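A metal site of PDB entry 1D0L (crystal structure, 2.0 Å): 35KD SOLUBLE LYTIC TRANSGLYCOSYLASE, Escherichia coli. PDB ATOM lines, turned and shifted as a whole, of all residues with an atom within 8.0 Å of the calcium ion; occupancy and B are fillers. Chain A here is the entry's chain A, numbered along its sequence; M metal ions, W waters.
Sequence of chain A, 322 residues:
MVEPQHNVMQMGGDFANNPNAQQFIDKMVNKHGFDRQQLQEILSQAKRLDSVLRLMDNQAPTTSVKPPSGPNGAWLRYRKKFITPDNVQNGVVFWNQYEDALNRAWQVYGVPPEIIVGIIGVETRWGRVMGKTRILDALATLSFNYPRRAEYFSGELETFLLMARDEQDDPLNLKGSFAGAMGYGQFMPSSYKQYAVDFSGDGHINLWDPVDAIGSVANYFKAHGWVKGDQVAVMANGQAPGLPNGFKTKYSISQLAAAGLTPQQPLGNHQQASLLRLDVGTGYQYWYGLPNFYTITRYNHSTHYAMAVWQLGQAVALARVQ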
ATOM      1  N   GLU A 167       6.311 -29.430  -7.918  1.00  0.00           N
ATOM      2  CA  GLU A 167       4.851 -29.374  -7.905  1.00  0.00           C
ATOM      3  C   GLU A 167       4.222 -30.760  -7.747  1.00  0.00           C
ATOM      4  O   GLU A 167       3.008 -30.915  -7.894  1.00  0.00           O
ATOM      5  CB  GLU A 167       4.317 -28.656  -9.150  1.00  0.00           C
ATOM      6  CG  GLU A 167       4.841 -27.205  -9.357  1.00  0.00           C
ATOM      7  CD  GLU A 167       4.276 -26.167  -8.366  1.00  0.00           C
ATOM      8  OE1 GLU A 167       3.968 -26.510  -7.198  1.00  0.00           O
ATOM      9  OE2 GLU A 167       4.148 -24.987  -8.769  1.00  0.00           O
ATOM     10  N   VAL A 197       4.436 -17.158 -13.538  1.00  0.00           N
ATOM     11  CA  VAL A 197       4.012 -16.585 -12.261  1.00  0.00           C
ATOM     12  C   VAL A 197       2.674 -17.172 -11.822  1.00  0.00           C
ATOM     13  O   VAL A 197       1.846 -17.583 -12.641  1.00  0.00           O
ATOM     14  CB  VAL A 197       3.855 -15.026 -12.340  1.00  0.00           C
ATOM     15  CG1 VAL A 197       5.194 -14.362 -12.635  1.00  0.00           C
ATOM     16  CG2 VAL A 197       2.851 -14.634 -13.392  1.00  0.00           C
ATOM     17  N   ASP A 198       2.478 -17.226 -10.504  1.00  0.00           N
ATOM     18  CA  ASP A 198       1.240 -17.711  -9.931  1.00  0.00           C
ATOM     19  C   ASP A 198       0.281 -16.516  -9.933  1.00  0.00           C
ATOM     20  O   ASP A 198       0.022 -15.908  -8.890  1.00  0.00           O
ATOM     21  CB  ASP A 198       1.485 -18.177  -8.495  1.00  0.00           C
ATOM     22  CG  ASP A 198       0.199 -18.482  -7.767  1.00  0.00           C
ATOM     23  OD1 ASP A 198      -0.776 -18.872  -8.432  1.00  0.00           O
ATOM     24  OD2 ASP A 198       0.157 -18.301  -6.534  1.00  0.00           O
ATOM     25  N   PHE A 199      -0.245 -16.176 -11.104  1.00  0.00           N
ATOM     26  CA  PHE A 199      -1.151 -15.046 -11.234  1.00  0.00           C
ATOM     27  C   PHE A 199      -2.523 -15.260 -10.595  1.00  0.00           C
ATOM     28  O   PHE A 199      -3.194 -14.289 -10.251  1.00  0.00           O
ATOM     29  CB  PHE A 199      -1.312 -14.668 -12.707  1.00  0.00           C
ATOM     30  CG  PHE A 199      -1.535 -13.203 -12.933  1.00  0.00           C
ATOM     31  CD1 PHE A 199      -0.645 -12.259 -12.426  1.00  0.00           C
ATOM     32  CD2 PHE A 199      -2.623 -12.750 -13.688  1.00  0.00           C
ATOM     33  CE1 PHE A 199      -0.833 -10.900 -12.652  1.00  0.00           C
ATOM     34  CE2 PHE A 199      -2.820 -11.390 -13.914  1.00  0.00           C
ATOM     35  CZ  PHE A 199      -1.925 -10.466 -13.401  1.00  0.00           C
ATOM     36  N   SER A 200      -2.937 -16.518 -10.439  1.00  0.00           N
ATOM     37  CA  SER A 200      -4.227 -16.826  -9.826  1.00  0.00           C
ATOM     38  C   SER A 200      -4.154 -16.703  -8.306  1.00  0.00           C
ATOM     39  O   SER A 200      -5.173 -16.598  -7.636  1.00  0.00           O
ATOM     40  CB  SER A 200      -4.725 -18.218 -10.235  1.00  0.00           C
ATOM     41  OG  SER A 200      -3.952 -19.236  -9.613  1.00  0.00           O
ATOM     42  N   GLY A 201      -2.940 -16.760  -7.770  1.00  0.00           N
ATOM     43  CA  GLY A 201      -2.745 -16.619  -6.331  1.00  0.00           C
ATOM     44  C   GLY A 201      -3.016 -17.803  -5.407  1.00  0.00           C
ATOM     45  O   GLY A 201      -3.146 -17.610  -4.208  1.00  0.00           O
ATOM     46  N   ASP A 202      -3.082 -19.011  -5.944  1.00  0.00           N
ATOM     47  CA  ASP A 202      -3.328 -20.195  -5.104  1.00  0.00           C
ATOM     48  C   ASP A 202      -2.030 -20.800  -4.558  1.00  0.00           C
ATOM     49  O   ASP A 202      -2.056 -21.833  -3.883  1.00  0.00           O
ATOM     50  CB  ASP A 202      -4.146 -21.238  -5.864  1.00  0.00           C
ATOM     51  CG  ASP A 202      -3.393 -21.836  -7.056  1.00  0.00           C
ATOM     52  OD1 ASP A 202      -2.368 -21.266  -7.494  1.00  0.00           O
ATOM     53  OD2 ASP A 202      -3.822 -22.878  -7.564  1.00  0.00           O
ATOM     54  N   GLY A 203      -0.912 -20.154  -4.853  1.00  0.00           N
ATOM     55  CA  GLY A 203       0.395 -20.618  -4.403  1.00  0.00           C
ATOM     56  C   GLY A 203       1.090 -21.578  -5.347  1.00  0.00           C
ATOM     57  O   GLY A 203       2.222 -21.992  -5.087  1.00  0.00           O
ATOM     58  N   HIS A 204       0.442 -21.903  -6.468  1.00  0.00           N
ATOM     59  CA  HIS A 204       1.010 -22.838  -7.438  1.00  0.00           C
ATOM     60  C   HIS A 204       1.030 -22.299  -8.870  1.00  0.00           C
ATOM     61  O   HIS A 204       0.049 -21.727  -9.329  1.00  0.00           O
ATOM     62  CB  HIS A 204       0.238 -24.157  -7.392  1.00  0.00           C
ATOM     63  CG  HIS A 204       0.386 -24.886  -6.083  1.00  0.00           C
ATOM     64  ND1 HIS A 204       1.244 -25.947  -5.911  1.00  0.00           N
ATOM     65  CD2 HIS A 204      -0.181 -24.663  -4.873  1.00  0.00           C
ATOM     66  CE1 HIS A 204       1.204 -26.353  -4.655  1.00  0.00           C
ATOM     67  NE2 HIS A 204       0.343 -25.596  -4.011  1.00  0.00           N
ATOM     68  N   ILE A 205       2.144 -22.487  -9.558  1.00  0.00           N
ATOM     69  CA  ILE A 205       2.261 -22.044 -10.942  1.00  0.00           C
ATOM     70  C   ILE A 205       1.828 -23.190 -11.857  1.00  0.00           C
ATOM     71  O   ILE A 205       2.520 -24.197 -11.991  1.00  0.00           O
ATOM     72  CB  ILE A 205       3.688 -21.576 -11.274  1.00  0.00           C
ATOM     73  CG1 ILE A 205       4.143 -20.532 -10.254  1.00  0.00           C
ATOM     74  CG2 ILE A 205       3.707 -20.946 -12.660  1.00  0.00           C
ATOM     75  CD1 ILE A 205       5.566 -20.053 -10.453  1.00  0.00           C
ATOM     76  N   ASN A 206       0.649 -23.036 -12.434  1.00  0.00           N
ATOM     77  CA  ASN A 206       0.043 -24.035 -13.296  1.00  0.00           C
ATOM     78  C   ASN A 206      -0.099 -23.478 -14.700  1.00  0.00           C
ATOM     79  O   ASN A 206      -0.950 -22.615 -14.947  1.00  0.00           O
ATOM     80  CB  ASN A 206      -1.326 -24.424 -12.730  1.00  0.00           C
ATOM     81  CG  ASN A 206      -2.011 -25.523 -13.528  1.00  0.00           C
ATOM     82  OD1 ASN A 206      -1.497 -26.001 -14.532  1.00  0.00           O
ATOM     83  ND2 ASN A 206      -3.198 -25.906 -13.071  1.00  0.00           N
ATOM     84  N   LEU A 207       0.686 -24.014 -15.629  1.00  0.00           N
ATOM     85  CA  LEU A 207       0.667 -23.584 -17.028  1.00  0.00           C
ATOM     86  C   LEU A 207      -0.658 -23.895 -17.730  1.00  0.00           C
ATOM     87  O   LEU A 207      -0.943 -23.346 -18.793  1.00  0.00           O
ATOM     88  CB  LEU A 207       1.832 -24.218 -17.788  1.00  0.00           C
ATOM     89  CG  LEU A 207       3.216 -23.791 -17.290  1.00  0.00           C
ATOM     90  CD1 LEU A 207       4.329 -24.581 -17.970  1.00  0.00           C
ATOM     91  CD2 LEU A 207       3.383 -22.290 -17.525  1.00  0.00           C
ATOM     92  N   ASP A 209      -3.586 -23.441 -16.165  1.00  0.00           N
ATOM     93  CA  ASP A 209      -4.590 -22.589 -15.506  1.00  0.00           C
ATOM     94  C   ASP A 209      -4.568 -21.312 -16.371  1.00  0.00           C
ATOM     95  O   ASP A 209      -3.545 -20.633 -16.465  1.00  0.00           O
ATOM     96  CB  ASP A 209      -4.148 -22.273 -14.064  1.00  0.00           C
ATOM     97  CG  ASP A 209      -5.152 -21.397 -13.297  1.00  0.00           C
ATOM     98  OD1 ASP A 209      -5.620 -20.373 -13.822  1.00  0.00           O
ATOM     99  OD2 ASP A 209      -5.443 -21.711 -12.127  1.00  0.00           O
ATOM    100  N   VAL A 211      -5.607 -18.292 -15.917  1.00  0.00           N
ATOM    101  CA  VAL A 211      -5.198 -17.073 -15.202  1.00  0.00           C
ATOM    102  C   VAL A 211      -3.670 -17.020 -15.021  1.00  0.00           C
ATOM    103  O   VAL A 211      -3.048 -15.981 -15.259  1.00  0.00           O
ATOM    104  CB  VAL A 211      -5.924 -16.927 -13.850  1.00  0.00           C
ATOM    105  CG1 VAL A 211      -5.439 -15.691 -13.121  1.00  0.00           C
ATOM    106  CG2 VAL A 211      -7.418 -16.817 -14.104  1.00  0.00           C
ATOM    107  N   ASP A 212      -3.076 -18.145 -14.614  1.00  0.00           N
ATOM    108  CA  ASP A 212      -1.625 -18.197 -14.451  1.00  0.00           C
ATOM    109  C   ASP A 212      -0.941 -17.962 -15.793  1.00  0.00           C
ATOM    110  O   ASP A 212       0.074 -17.268 -15.881  1.00  0.00           O
ATOM    111  CB  ASP A 212      -1.189 -19.577 -13.952  1.00  0.00           C
ATOM    112  CG  ASP A 212      -1.394 -19.758 -12.458  1.00  0.00           C
ATOM    113  OD1 ASP A 212      -1.993 -18.888 -11.792  1.00  0.00           O
ATOM    114  OD2 ASP A 212      -0.929 -20.794 -11.940  1.00  0.00           O
ATOM    115  N   ALA A 213      -1.503 -18.557 -16.843  1.00  0.00           N
ATOM    116  CA  ALA A 213      -0.943 -18.412 -18.197  1.00  0.00           C
ATOM    117  C   ALA A 213      -0.972 -16.956 -18.634  1.00  0.00           C
ATOM    118  O   ALA A 213      -0.010 -16.461 -19.194  1.00  0.00           O
ATOM    119  CB  ALA A 213      -1.722 -19.298 -19.185  1.00  0.00           C
HETATM  120 CA    CA M   1      -1.906 -20.520  -9.732  1.00  0.00          CA
HETATM  121  O   HOH W   1      -3.286 -22.221 -10.436  1.00  0.00           O
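OE1 of Glu 167 lies within hydrogen-bond range of ND1 of His 204 (3.1 Å). The backbone NH of Gly 201 lies close to the side-chain carboxylate of Asp 198 (3.1 Å). The side-chain carboxylate of Asp 198 lies within hydrogen-bond range of the backbone NH of Gly 203 (2.7 Å). OD1 of Asp 209 sits at hydrogen-bond distance from N of Asp 212 (3.5 Å). The side-chain carboxylate (OD2) of Asp 212 sits close to the backbone NH (N) of Asn 206, at 2.8 Å. N of Phe 199 sits close to OD1 of Asp 212, at 3.3 Å.
Five residues have an atom within 4 Å of the calcium ion: Asp 198, Ser 200, Asp 202, His 204 and Asp 212. Along chain A the residues within 4 Å of the calcium ion span positions 198 to 212. The nearest printed residue that does not touch the calcium ion is Gly 201 (4.4 Å).
The calcium ion is bound by water W1, O of His 204, OD1 of Asp 198, OD1 of Asp 202, OG of Ser 200, OD2 of Asp 212 and OD1 of Asp 212. The calcium ion has seven donor atoms within binding distance.
Water W1 bridges OD2 of Asp 209 (2.8 Å) and OD2 of Asp 202 (3.0 Å).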
